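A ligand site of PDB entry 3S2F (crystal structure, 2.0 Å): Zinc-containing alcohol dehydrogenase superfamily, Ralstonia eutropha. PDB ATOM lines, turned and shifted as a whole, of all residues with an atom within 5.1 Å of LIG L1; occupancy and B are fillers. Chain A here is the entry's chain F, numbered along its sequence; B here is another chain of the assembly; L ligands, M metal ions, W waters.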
ATOM      1  N   CYS A  40      15.954  18.072  19.694  1.00  0.00           N
ATOM      2  CA  CYS A  40      16.053  17.504  21.032  1.00  0.00           C
ATOM      3  C   CYS A  40      15.188  16.267  21.160  1.00  0.00           C
ATOM      4  O   CYS A  40      14.123  16.166  20.546  1.00  0.00           O
ATOM      5  CB  CYS A  40      15.650  18.536  22.086  1.00  0.00           C
ATOM      6  SG  CYS A  40      15.779  17.874  23.775  1.00  0.00           S
ATOM      7  N   HIS A  41      15.652  15.304  21.952  1.00  0.00           N
ATOM      8  CA  HIS A  41      14.907  14.078  22.169  1.00  0.00           C
ATOM      9  C   HIS A  41      13.512  14.395  22.691  1.00  0.00           C
ATOM     10  O   HIS A  41      12.572  13.633  22.494  1.00  0.00           O
ATOM     11  CB  HIS A  41      15.632  13.162  23.145  1.00  0.00           C
ATOM     12  CG  HIS A  41      15.201  11.733  23.072  1.00  0.00           C
ATOM     13  ND1 HIS A  41      13.936  11.316  23.432  1.00  0.00           N
ATOM     14  CD2 HIS A  41      15.862  10.624  22.661  1.00  0.00           C
ATOM     15  CE1 HIS A  41      13.839  10.015  23.257  1.00  0.00           C
ATOM     16  NE2 HIS A  41      14.996   9.569  22.791  1.00  0.00           N
ATOM     17  N   THR A  42      13.398  15.530  23.379  1.00  0.00           N
ATOM     18  CA  THR A  42      12.119  15.997  23.890  1.00  0.00           C
ATOM     19  C   THR A  42      11.115  16.174  22.756  1.00  0.00           C
ATOM     20  O   THR A  42       9.929  15.905  22.915  1.00  0.00           O
ATOM     21  CB  THR A  42      12.268  17.328  24.632  1.00  0.00           C
ATOM     22  OG1 THR A  42      12.748  17.098  25.957  1.00  0.00           O
ATOM     23  CG2 THR A  42      10.922  18.050  24.702  1.00  0.00           C
ATOM     24  N   TRP A  51       3.304  12.883  26.644  1.00  0.00           N
ATOM     25  CA  TRP A  51       3.407  13.295  28.050  1.00  0.00           C
ATOM     26  C   TRP A  51       2.089  13.655  28.738  1.00  0.00           C
ATOM     27  O   TRP A  51       1.102  13.969  28.075  1.00  0.00           O
ATOM     28  CB  TRP A  51       4.389  14.457  28.172  1.00  0.00           C
ATOM     29  CG  TRP A  51       5.816  14.047  27.969  1.00  0.00           C
ATOM     30  CD1 TRP A  51       6.302  12.769  27.938  1.00  0.00           C
ATOM     31  CD2 TRP A  51       6.947  14.909  27.772  1.00  0.00           C
ATOM     32  NE1 TRP A  51       7.665  12.791  27.744  1.00  0.00           N
ATOM     33  CE2 TRP A  51       8.082  14.091  27.632  1.00  0.00           C
ATOM     34  CE3 TRP A  51       7.097  16.297  27.699  1.00  0.00           C
ATOM     35  CZ2 TRP A  51       9.352  14.611  27.424  1.00  0.00           C
ATOM     36  CZ3 TRP A  51       8.364  16.808  27.490  1.00  0.00           C
ATOM     37  CH2 TRP A  51       9.471  15.967  27.352  1.00  0.00           C
ATOM     38  N   CYS A 150      19.564  24.105  24.557  1.00  0.00           N
ATOM     39  CA  CYS A 150      18.889  23.191  25.469  1.00  0.00           C
ATOM     40  C   CYS A 150      19.830  22.119  26.032  1.00  0.00           C
ATOM     41  O   CYS A 150      19.950  21.973  27.240  1.00  0.00           O
ATOM     42  CB  CYS A 150      17.677  22.527  24.813  1.00  0.00           C
ATOM     43  SG  CYS A 150      16.627  21.700  26.020  1.00  0.00           S
ATOM     44  N   THR A 154      21.072  22.938  29.842  1.00  0.00           N
ATOM     45  CA  THR A 154      20.467  21.956  30.736  1.00  0.00           C
ATOM     46  C   THR A 154      21.510  21.208  31.581  1.00  0.00           C
ATOM     47  O   THR A 154      21.420  21.194  32.812  1.00  0.00           O
ATOM     48  CB  THR A 154      19.596  20.934  29.984  1.00  0.00           C
ATOM     49  OG1 THR A 154      18.508  21.616  29.358  1.00  0.00           O
ATOM     50  CG2 THR A 154      19.058  19.879  30.932  1.00  0.00           C
ATOM     51  N   SER A 173      25.470   9.795  32.908  1.00  0.00           N
ATOM     52  CA  SER A 173      24.713   8.655  32.412  1.00  0.00           C
ATOM     53  C   SER A 173      23.935   9.046  31.156  1.00  0.00           C
ATOM     54  O   SER A 173      23.063   9.912  31.199  1.00  0.00           O
ATOM     55  CB  SER A 173      23.751   8.139  33.475  1.00  0.00           C
ATOM     56  OG  SER A 173      22.909   7.130  32.949  1.00  0.00           O
ATOM     57  N   GLY A 174      24.258   8.392  30.053  1.00  0.00           N
ATOM     58  CA  GLY A 174      23.658   8.738  28.778  1.00  0.00           C
ATOM     59  C   GLY A 174      24.515   9.749  28.058  1.00  0.00           C
ATOM     60  O   GLY A 174      24.524  10.929  28.410  1.00  0.00           O
ATOM     61  N   ILE A 175      25.270   9.286  27.060  1.00  0.00           N
ATOM     62  CA  ILE A 175      26.133  10.169  26.294  1.00  0.00           C
ATOM     63  C   ILE A 175      25.506  10.499  24.950  1.00  0.00           C
ATOM     64  O   ILE A 175      26.028  10.141  23.902  1.00  0.00           O
ATOM     65  CB  ILE A 175      27.531   9.557  26.085  1.00  0.00           C
ATOM     66  CG1 ILE A 175      28.043   8.941  27.386  1.00  0.00           C
ATOM     67  CG2 ILE A 175      28.499  10.596  25.551  1.00  0.00           C
ATOM     68  CD1 ILE A 175      28.141   9.936  28.530  1.00  0.00           C
ATOM     69  N   GLY A 176      24.355  11.171  24.995  1.00  0.00           N
ATOM     70  CA  GLY A 176      23.668  11.588  23.785  1.00  0.00           C
ATOM     71  C   GLY A 176      23.807  13.079  23.555  1.00  0.00           C
ATOM     72  O   GLY A 176      24.882  13.649  23.769  1.00  0.00           O
ATOM     73  N   GLY A 177      22.725  13.710  23.116  1.00  0.00           N
ATOM     74  CA  GLY A 177      22.709  15.151  22.905  1.00  0.00           C
ATOM     75  C   GLY A 177      23.149  15.899  24.152  1.00  0.00           C
ATOM     76  O   GLY A 177      24.115  16.661  24.113  1.00  0.00           O
ATOM     77  N   LEU A 178      22.437  15.683  25.249  1.00  0.00           N
ATOM     78  CA  LEU A 178      22.789  16.278  26.532  1.00  0.00           C
ATOM     79  C   LEU A 178      24.131  15.747  27.018  1.00  0.00           C
ATOM     80  O   LEU A 178      25.016  16.517  27.387  1.00  0.00           O
ATOM     81  CB  LEU A 178      21.731  15.960  27.591  1.00  0.00           C
ATOM     82  CG  LEU A 178      20.270  16.370  27.435  1.00  0.00           C
ATOM     83  CD1 LEU A 178      19.751  17.042  28.705  1.00  0.00           C
ATOM     84  CD2 LEU A 178      20.051  17.263  26.226  1.00  0.00           C
ATOM     85  N   GLY A 179      24.270  14.427  27.022  1.00  0.00           N
ATOM     86  CA  GLY A 179      25.398  13.761  27.652  1.00  0.00           C
ATOM     87  C   GLY A 179      26.775  14.118  27.118  1.00  0.00           C
ATOM     88  O   GLY A 179      27.691  14.369  27.899  1.00  0.00           O
ATOM     89  N   VAL A 196      28.612   6.538  31.334  1.00  0.00           N
ATOM     90  CA  VAL A 196      27.801   5.330  31.246  1.00  0.00           C
ATOM     91  C   VAL A 196      26.826   5.402  30.077  1.00  0.00           C
ATOM     92  O   VAL A 196      26.183   6.429  29.851  1.00  0.00           O
ATOM     93  CB  VAL A 196      27.015   5.082  32.533  1.00  0.00           C
ATOM     94  CG1 VAL A 196      26.274   3.750  32.458  1.00  0.00           C
ATOM     95  CG2 VAL A 196      27.939   5.112  33.743  1.00  0.00           C
ATOM     96  N   ASP A 197      26.749   4.302  29.337  1.00  0.00           N
ATOM     97  CA  ASP A 197      25.780   4.161  28.254  1.00  0.00           C
ATOM     98  C   ASP A 197      25.648   2.682  27.920  1.00  0.00           C
ATOM     99  O   ASP A 197      26.184   1.827  28.641  1.00  0.00           O
ATOM    100  CB  ASP A 197      26.219   4.966  27.025  1.00  0.00           C
ATOM    101  CG  ASP A 197      25.035   5.535  26.256  1.00  0.00           C
ATOM    102  OD1 ASP A 197      24.121   4.753  25.913  1.00  0.00           O
ATOM    103  OD2 ASP A 197      25.008   6.758  26.008  1.00  0.00           O
ATOM    104  N   ILE A 198      24.940   2.366  26.847  1.00  0.00           N
ATOM    105  CA  ILE A 198      24.656   0.980  26.483  1.00  0.00           C
ATOM    106  C   ILE A 198      25.213   0.624  25.114  1.00  0.00           C
ATOM    107  O   ILE A 198      24.777  -0.338  24.487  1.00  0.00           O
ATOM    108  CB  ILE A 198      23.145   0.720  26.472  1.00  0.00           C
ATOM    109  CG1 ILE A 198      22.456   1.677  25.494  1.00  0.00           C
ATOM    110  CG2 ILE A 198      22.565   0.868  27.863  1.00  0.00           C
ATOM    111  CD1 ILE A 198      20.947   1.614  25.549  1.00  0.00           C
ATOM    112  N   LYS A 202      29.184   5.245  21.826  1.00  0.00           N
ATOM    113  CA  LYS A 202      28.823   6.424  22.593  1.00  0.00           C
ATOM    114  C   LYS A 202      29.809   6.650  23.739  1.00  0.00           C
ATOM    115  O   LYS A 202      30.121   7.791  24.084  1.00  0.00           O
ATOM    116  CB  LYS A 202      27.384   6.319  23.104  1.00  0.00           C
ATOM    117  CG  LYS A 202      26.369   6.080  21.983  1.00  0.00           C
ATOM    118  CD  LYS A 202      24.936   6.015  22.500  1.00  0.00           C
ATOM    119  CE  LYS A 202      23.972   5.639  21.384  1.00  0.00           C
ATOM    120  NZ  LYS A 202      23.968   6.625  20.264  1.00  0.00           N
ATOM    121  N   ALA A 217      26.612  -0.397  30.305  1.00  0.00           N
ATOM    122  CA  ALA A 217      25.642  -0.974  31.234  1.00  0.00           C
ATOM    123  C   ALA A 217      25.000  -2.251  30.696  1.00  0.00           C
ATOM    124  O   ALA A 217      24.313  -2.952  31.429  1.00  0.00           O
ATOM    125  CB  ALA A 217      24.576   0.048  31.581  1.00  0.00           C
ATOM    126  N   THR A 239      21.059  11.732  32.063  1.00  0.00           N
ATOM    127  CA  THR A 239      20.397  12.234  30.872  1.00  0.00           C
ATOM    128  C   THR A 239      19.770  11.078  30.101  1.00  0.00           C
ATOM    129  O   THR A 239      19.116  11.285  29.064  1.00  0.00           O
ATOM    130  CB  THR A 239      21.368  12.992  29.954  1.00  0.00           C
ATOM    131  OG1 THR A 239      22.222  12.056  29.287  1.00  0.00           O
ATOM    132  CG2 THR A 239      22.218  13.975  30.756  1.00  0.00           C
ATOM    133  N   ALA A 240      19.961   9.858  30.590  1.00  0.00           N
ATOM    134  CA  ALA A 240      19.505   8.651  29.893  1.00  0.00           C
ATOM    135  C   ALA A 240      18.001   8.622  29.671  1.00  0.00           C
ATOM    136  O   ALA A 240      17.230   9.205  30.443  1.00  0.00           O
ATOM    137  CB  ALA A 240      19.967   7.403  30.646  1.00  0.00           C
ATOM    138  N   VAL A 241      17.575   7.939  28.610  1.00  0.00           N
ATOM    139  CA  VAL A 241      16.166   7.794  28.291  1.00  0.00           C
ATOM    140  C   VAL A 241      15.673   6.395  28.666  1.00  0.00           C
ATOM    141  O   VAL A 241      15.030   5.707  27.876  1.00  0.00           O
ATOM    142  CB  VAL A 241      15.880   8.060  26.800  1.00  0.00           C
ATOM    143  CG1 VAL A 241      16.130   9.538  26.478  1.00  0.00           C
ATOM    144  CG2 VAL A 241      16.739   7.161  25.929  1.00  0.00           C
ATOM    145  N   SER A 242      15.985   5.990  29.897  1.00  0.00           N
ATOM    146  CA  SER A 242      15.583   4.694  30.414  1.00  0.00           C
ATOM    147  C   SER A 242      15.465   4.763  31.928  1.00  0.00           C
ATOM    148  O   SER A 242      16.420   5.115  32.613  1.00  0.00           O
ATOM    149  CB  SER A 242      16.596   3.620  30.028  1.00  0.00           C
ATOM    150  OG  SER A 242      16.348   2.411  30.732  1.00  0.00           O
ATOM    151  N   LYS A 244      15.464   2.455  33.985  1.00  0.00           N
ATOM    152  CA  LYS A 244      16.461   1.545  34.541  1.00  0.00           C
ATOM    153  C   LYS A 244      17.726   2.295  34.950  1.00  0.00           C
ATOM    154  O   LYS A 244      18.240   2.103  36.054  1.00  0.00           O
ATOM    155  CB  LYS A 244      16.799   0.472  33.506  1.00  0.00           C
ATOM    156  CG  LYS A 244      17.415  -0.789  34.094  1.00  0.00           C
ATOM    157  CD  LYS A 244      17.813  -1.750  32.980  1.00  0.00           C
ATOM    158  CE  LYS A 244      16.620  -2.157  32.124  1.00  0.00           C
ATOM    159  NZ  LYS A 244      17.040  -2.915  30.916  1.00  0.00           N
ATOM    160  N   ALA A 245      18.203   3.165  34.057  1.00  0.00           N
ATOM    161  CA  ALA A 245      19.416   3.937  34.304  1.00  0.00           C
ATOM    162  C   ALA A 245      19.302   4.856  35.529  1.00  0.00           C
ATOM    163  O   ALA A 245      20.308   5.193  36.146  1.00  0.00           O
ATOM    164  CB  ALA A 245      19.768   4.754  33.067  1.00  0.00           C
ATOM    165  N   GLN A 248      19.927   2.572  38.555  1.00  0.00           N
ATOM    166  CA  GLN A 248      21.341   2.222  38.596  1.00  0.00           C
ATOM    167  C   GLN A 248      22.218   3.395  39.049  1.00  0.00           C
ATOM    168  O   GLN A 248      23.233   3.189  39.714  1.00  0.00           O
ATOM    169  CB  GLN A 248      21.814   1.726  37.223  1.00  0.00           C
ATOM    170  CG  GLN A 248      21.288   0.347  36.857  1.00  0.00           C
ATOM    171  CD  GLN A 248      21.607  -0.042  35.436  1.00  0.00           C
ATOM    172  OE1 GLN A 248      21.690   0.806  34.542  1.00  0.00           O
ATOM    173  NE2 GLN A 248      21.784  -1.336  35.206  1.00  0.00           N
ATOM    174  N   LEU A 261      18.854  14.803  38.013  1.00  0.00           N
ATOM    175  CA  LEU A 261      18.055  14.132  36.982  1.00  0.00           C
ATOM    176  C   LEU A 261      17.611  15.060  35.866  1.00  0.00           C
ATOM    177  O   LEU A 261      16.979  16.086  36.108  1.00  0.00           O
ATOM    178  CB  LEU A 261      16.830  13.474  37.604  1.00  0.00           C
ATOM    179  CG  LEU A 261      17.073  12.541  38.790  1.00  0.00           C
ATOM    180  CD1 LEU A 261      15.745  12.024  39.347  1.00  0.00           C
ATOM    181  CD2 LEU A 261      17.993  11.384  38.413  1.00  0.00           C
ATOM    182  N   ASN A 262      17.929  14.687  34.636  1.00  0.00           N
ATOM    183  CA  ASN A 262      17.518  15.446  33.461  1.00  0.00           C
ATOM    184  C   ASN A 262      16.588  14.642  32.553  1.00  0.00           C
ATOM    185  O   ASN A 262      15.616  15.177  32.008  1.00  0.00           O
ATOM    186  CB  ASN A 262      18.733  15.919  32.662  1.00  0.00           C
ATOM    187  CG  ASN A 262      19.329  17.201  33.223  1.00  0.00           C
ATOM    188  OD1 ASN A 262      18.645  17.977  33.873  1.00  0.00           O
ATOM    189  ND2 ASN A 262      20.617  17.408  32.966  1.00  0.00           N
ATOM    190  N   GLY A 263      16.903  13.365  32.397  1.00  0.00           N
ATOM    191  CA  GLY A 263      16.161  12.488  31.504  1.00  0.00           C
ATOM    192  C   GLY A 263      14.668  12.454  31.790  1.00  0.00           C
ATOM    193  O   GLY A 263      14.241  12.630  32.928  1.00  0.00           O
ATOM    194  N   LEU A 264      13.882  12.229  30.752  1.00  0.00           N
ATOM    195  CA  LEU A 264      12.438  12.210  30.893  1.00  0.00           C
ATOM    196  C   LEU A 264      11.762  11.009  30.229  1.00  0.00           C
ATOM    197  O   LEU A 264      10.801  11.171  29.469  1.00  0.00           O
ATOM    198  CB  LEU A 264      11.829  13.515  30.385  1.00  0.00           C
ATOM    199  CG  LEU A 264      12.127  14.749  31.219  1.00  0.00           C
ATOM    200  CD1 LEU A 264      11.872  16.018  30.430  1.00  0.00           C
ATOM    201  CD2 LEU A 264      11.298  14.734  32.495  1.00  0.00           C
ATOM    202  N   SER A 286      16.453  18.483  37.840  1.00  0.00           N
ATOM    203  CA  SER A 286      16.959  19.740  37.312  1.00  0.00           C
ATOM    204  C   SER A 286      16.268  20.029  35.986  1.00  0.00           C
ATOM    205  O   SER A 286      16.137  19.150  35.142  1.00  0.00           O
ATOM    206  CB  SER A 286      18.477  19.671  37.117  1.00  0.00           C
ATOM    207  OG  SER A 286      19.022  20.964  36.888  1.00  0.00           O
ATOM    208  N   ILE A 287      15.818  21.266  35.824  1.00  0.00           N
ATOM    209  CA  ILE A 287      14.992  21.612  34.677  1.00  0.00           C
ATOM    210  C   ILE A 287      15.582  22.745  33.846  1.00  0.00           C
ATOM    211  O   ILE A 287      15.617  23.898  34.281  1.00  0.00           O
ATOM    212  CB  ILE A 287      13.553  21.975  35.114  1.00  0.00           C
ATOM    213  CG1 ILE A 287      12.736  22.471  33.929  1.00  0.00           C
ATOM    214  CG2 ILE A 287      13.582  22.984  36.267  1.00  0.00           C
ATOM    215  CD1 ILE A 287      12.359  21.387  32.952  1.00  0.00           C
ATOM    216  N   VAL A 288      16.019  22.411  32.635  1.00  0.00           N
ATOM    217  CA  VAL A 288      16.792  23.304  31.779  1.00  0.00           C
ATOM    218  C   VAL A 288      17.664  24.257  32.580  1.00  0.00           C
ATOM    219  O   VAL A 288      18.404  23.825  33.472  1.00  0.00           O
ATOM    220  CB  VAL A 288      15.899  24.103  30.791  1.00  0.00           C
ATOM    221  CG1 VAL A 288      15.351  23.189  29.708  1.00  0.00           C
ATOM    222  CG2 VAL A 288      14.780  24.834  31.517  1.00  0.00           C
ATOM    223  N   LEU A 325      17.177   8.958  15.893  1.00  0.00           N
ATOM    224  CA  LEU A 325      17.274   9.352  17.297  1.00  0.00           C
ATOM    225  C   LEU A 325      16.602   8.310  18.186  1.00  0.00           C
ATOM    226  O   LEU A 325      17.164   7.872  19.193  1.00  0.00           O
ATOM    227  CB  LEU A 325      16.621  10.710  17.519  1.00  0.00           C
ATOM    228  CG  LEU A 325      17.362  11.764  18.349  1.00  0.00           C
ATOM    229  CD1 LEU A 325      16.383  12.524  19.245  1.00  0.00           C
ATOM    230  CD2 LEU A 325      18.462  11.125  19.179  1.00  0.00           C
ATOM    231  N   GLY A 332      25.820  12.268  19.180  1.00  0.00           N
ATOM    232  CA  GLY A 332      25.648  13.608  19.730  1.00  0.00           C
ATOM    233  C   GLY A 332      24.325  14.222  19.316  1.00  0.00           C
ATOM    234  O   GLY A 332      23.256  13.701  19.642  1.00  0.00           O
ATOM    235  N   ARG A 333      24.404  15.327  18.583  1.00  0.00           N
ATOM    236  CA  ARG A 333      23.218  16.080  18.202  1.00  0.00           C
ATOM    237  C   ARG A 333      23.025  16.129  16.691  1.00  0.00           C
ATOM    238  O   ARG A 333      24.000  16.175  15.928  1.00  0.00           O
ATOM    239  CB  ARG A 333      23.332  17.516  18.742  1.00  0.00           C
ATOM    240  CG  ARG A 333      22.536  17.789  20.008  1.00  0.00           C
ATOM    241  CD  ARG A 333      21.066  17.989  19.703  1.00  0.00           C
ATOM    242  NE  ARG A 333      20.373  18.610  20.829  1.00  0.00           N
ATOM    243  CZ  ARG A 333      19.730  17.939  21.776  1.00  0.00           C
ATOM    244  NH1 ARG A 333      19.138  18.587  22.767  1.00  0.00           N
ATOM    245  NH2 ARG A 333      19.687  16.617  21.730  1.00  0.00           N
ATOM    246  N   VAL B 277      11.627  15.837  37.968  1.00  0.00           N
ATOM    247  CA  VAL B 277      12.464  16.634  37.069  1.00  0.00           C
ATOM    248  C   VAL B 277      11.814  17.983  36.735  1.00  0.00           C
ATOM    249  O   VAL B 277      12.419  19.033  36.950  1.00  0.00           O
ATOM    250  CB  VAL B 277      12.778  15.882  35.762  1.00  0.00           C
ATOM    251  CG1 VAL B 277      13.481  16.792  34.769  1.00  0.00           C
ATOM    252  CG2 VAL B 277      13.594  14.634  36.052  1.00  0.00           C
HETATM  253  P1  LIG L   1      19.090  11.176  23.536  1.00  0.00           P
HETATM  254  O1  LIG L   1      20.163  12.002  22.762  1.00  0.00           O
HETATM  255  O2  LIG L   1      18.888  10.467  22.155  1.00  0.00           O
HETATM  256  O3  LIG L   1      20.302  10.660  24.444  1.00  0.00           O
HETATM  257  C1  LIG L   1      20.280   9.279  24.748  1.00  0.00           C
HETATM  258  C2  LIG L   1      21.296   8.836  25.800  1.00  0.00           C
HETATM  259  O4  LIG L   1      20.689   7.978  26.758  1.00  0.00           O
HETATM  260  C3  LIG L   1      22.393   8.030  25.160  1.00  0.00           C
HETATM  261  O5  LIG L   1      22.402   8.196  23.777  1.00  0.00           O
HETATM  262  C4  LIG L   1      22.048   6.616  25.423  1.00  0.00           C
HETATM  263  O6  LIG L   1      21.938   5.997  24.201  1.00  0.00           O
HETATM  264  C5  LIG L   1      20.749   6.709  26.122  1.00  0.00           C
HETATM  265  N1  LIG L   1      20.499   5.553  26.971  1.00  0.00           N
HETATM  266  C6  LIG L   1      19.488   4.677  26.782  1.00  0.00           C
HETATM  267  N2  LIG L   1      19.461   3.769  27.745  1.00  0.00           N
HETATM  268  C7  LIG L   1      20.468   4.001  28.595  1.00  0.00           C
HETATM  269  C8  LIG L   1      20.917   3.390  29.756  1.00  0.00           C
HETATM  270  N3  LIG L   1      20.247   2.227  30.289  1.00  0.00           N
HETATM  271  N4  LIG L   1      21.977   3.887  30.400  1.00  0.00           N
HETATM  272  C9  LIG L   1      22.629   4.985  29.954  1.00  0.00           C
HETATM  273  N5  LIG L   1      22.212   5.604  28.818  1.00  0.00           N
HETATM  274  C10 LIG L   1      21.146   5.156  28.132  1.00  0.00           C
HETATM  275  O7  LIG L   1      18.351  12.594  23.696  1.00  0.00           O
HETATM  276  P2  LIG L   1      18.758  13.811  24.616  1.00  0.00           P
HETATM  277  O8  LIG L   1      20.218  13.750  24.979  1.00  0.00           O
HETATM  278  O9  LIG L   1      18.506  15.089  23.828  1.00  0.00           O
HETATM  279  O10 LIG L   1      17.873  13.857  25.927  1.00  0.00           O
HETATM  280  C11 LIG L   1      17.412  12.691  26.565  1.00  0.00           C
HETATM  281  C12 LIG L   1      16.658  13.113  27.795  1.00  0.00           C
HETATM  282  O11 LIG L   1      16.872  14.478  27.953  1.00  0.00           O
HETATM  283  C13 LIG L   1      15.191  12.900  27.657  1.00  0.00           C
HETATM  284  O12 LIG L   1      14.898  12.451  26.396  1.00  0.00           O
HETATM  285  C14 LIG L   1      14.563  14.226  27.888  1.00  0.00           C
HETATM  286  O13 LIG L   1      14.223  14.779  26.680  1.00  0.00           O
HETATM  287  C15 LIG L   1      15.686  14.957  28.537  1.00  0.00           C
HETATM  288  N6  LIG L   1      15.694  16.414  28.531  1.00  0.00           N
HETATM  289  C16 LIG L   1      15.536  17.084  29.722  1.00  0.00           C
HETATM  290  C17 LIG L   1      15.687  18.469  29.794  1.00  0.00           C
HETATM  291  C18 LIG L   1      15.482  19.078  31.153  1.00  0.00           C
HETATM  292  O14 LIG L   1      15.645  20.279  31.336  1.00  0.00           O
HETATM  293  N7  LIG L   1      15.117  18.204  32.237  1.00  0.00           N
HETATM  294  C19 LIG L   1      16.030  19.195  28.669  1.00  0.00           C
HETATM  295  C20 LIG L   1      16.203  18.509  27.471  1.00  0.00           C
HETATM  296  C21 LIG L   1      16.045  17.125  27.411  1.00  0.00           C
HETATM  297  C1  LG2 L   2      13.735  20.176  27.148  1.00  0.00           C
HETATM  298  C2  LG2 L   2      12.643  19.984  28.133  1.00  0.00           C
HETATM  299  O1  LG2 L   2      11.518  19.287  27.867  1.00  0.00           O
HETATM  300  C3  LG2 L   2      10.768  19.319  28.986  1.00  0.00           C
HETATM  301  C4  LG2 L   2      11.418  20.040  29.978  1.00  0.00           C
HETATM  302  C5  LG2 L   2      12.627  20.462  29.433  1.00  0.00           C
HETATM  303  O2  LG2 L   2      13.594  19.733  26.017  1.00  0.00           O
HETATM  304 ZN    ZN M   1      15.366  20.033  24.749  1.00  0.00          ZN
HETATM  305  O   HOH W   1      20.406   3.691  22.570  1.00  0.00           O
HETATM  306  O   HOH W   2      18.888   8.194  21.084  1.00  0.00           O
HETATM  307  O   HOH W   3      12.301  11.252  26.526  1.00  0.00           O
HETATM  308  O   HOH W   4      18.457   0.399  28.346  1.00  0.00           O
HETATM  309  O   HOH W   5      23.629   8.912  21.546  1.00  0.00           O
HETATM  310  O   HOH W   6      22.851   2.823  33.110  1.00  0.00           O
HETATM  311  O   HOH W   7      20.754   0.188  32.071  1.00  0.00           O
HETATM  312  O   HOH W   8      22.169  12.457  26.530  1.00  0.00           O
HETATM  313  O   HOH W   9      22.276  10.930  20.667  1.00  0.00           O
HETATM  314  O   HOH W  10      20.766  14.214  20.258  1.00  0.00           O
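The backbone carbonyl oxygen (O) of Ser 173 lies within hydrogen-bond range of the backbone NH (N) of Ala 240 (3.2 Å). The side-chain carboxylate of Asp 197 is in hydrogen-bond range of the backbone NH of Ile 175 (2.8 Å). O of Gly 174 lies within hydrogen-bond range of OG1 of Thr 239. O of Ser 173 lies within hydrogen-bond range of N of Thr 239. The backbone carbonyl oxygen (O) of Leu 261 lies within hydrogen-bond range of the backbone NH (N) of Ser 286, at 3.0 Å. The side-chain sulfur of Cys 40 sits close to the backbone NH of Thr 42, at 3.4 Å. The guanidinium group of Arg 333 lies close to the side-chain sulfur of Cys 40, at 3.6 Å. The side-chain amide oxygen (OD1) of Asn 262 sits close to the backbone carbonyl oxygen (O) of Ser 286 (3.0 Å).
O9 of LIG L1 is in salt-bridge range of NH2 of Arg 333. O of Ser 286 lies within hydrogen-bond range of N7 of LIG L1 (3.2 Å). The backbone carbonyl oxygen (O) of Asn 262 lies close to a nitrogen (N7) of LIG L1, at 3.1 Å. The backbone NH (N) of Thr 42 sits at hydrogen-bond distance from an oxygen (O13) of LIG L1, at 3.5 Å. An oxygen (O14) of LIG L1 is in hydrogen-bond range of the backbone NH of Val 288 (2.5 Å). The side-chain carboxylate (OD1) of Asp 197 sits close to an oxygen (O6) of LIG L1, at 3.0 Å. The backbone NH (N) of Gly 177 lies within hydrogen-bond range of an oxygen (O1) of LIG L1 (3.1 Å). The side-chain hydroxyl (OG1) of Thr 42 lies within hydrogen-bond range of an oxygen (O1) of LG2 L2 (3.2 Å). N of His 41 sits at hydrogen-bond distance from O9 of LIG L1, at 3.4 Å. ND1 of His 41 lies within hydrogen-bond range of O12 of LIG L1 (3.3 Å). N of Leu 178 is in hydrogen-bond range of O8 of LIG L1 (3.0 Å). The side-chain hydroxyl (OG1) of Thr 42 sits at hydrogen-bond distance from an oxygen (O13) of LIG L1 (2.8 Å).
Water W2 lies within hydrogen-bond range of O2 of LIG L1 (2.5 Å) and O of Leu 325 (2.6 Å). Water W5 lies within hydrogen-bond range of NZ of Lys 202 and O5 of LIG L1. Water W7 bridges the side-chain amide oxygen (OE1) of Gln 248 (2.7 Å) and a nitrogen (N3) of LIG L1 (2.8 Å). Water W6 bridges the side-chain amide oxygen of Gln 248 (2.7 Å) and a nitrogen (N4) of LIG L1 (3.0 Å). Water W9 bridges O of Gly 332 (3.1 Å) and O1 of LIG L1 (3.2 Å). Water W10 lies within hydrogen-bond range of the backbone carbonyl oxygen of Gly 332 (2.6 Å), the guanidinium group of Arg 333 (3.0 Å) and an oxygen (O1) of LIG L1 (3.4 Å).
Merely in contact with LIG L1: Cys 40 (3.7 Å), Cys 150 (3.5 Å), Thr 154 (3.5 Å), Ser 173 (3.7 Å), Gly 174 (3.5 Å), Ile 175 (3.7 Å), Gly 176 (3.6 Å), Val 196 (3.8 Å), Ile 198 (3.4 Å), Lys 202 (3.4 Å), Thr 239 (3.3 Å), Ala 240 (3.4 Å), Val 241 (3.2 Å), Ser 242 (3.7 Å), Ala 245 (3.6 Å), Gly 263 (3.8 Å), Leu 264 (3.4 Å), Ile 287 (3.5 Å), Leu 325 (3.1 Å) and Val 277 of chain B (3.3 Å). Hydrophobic or aromatic side chains within 4 Å of LIG L1: His 41, Leu 178, Ile 198, Ala 240, Val 241, Ala 245, Leu 264, Ile 287, Val 288, Leu 325 and Val 277 of chain B. Along chain A the residues within 4 Å of LIG L1 span positions 40 to 333.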
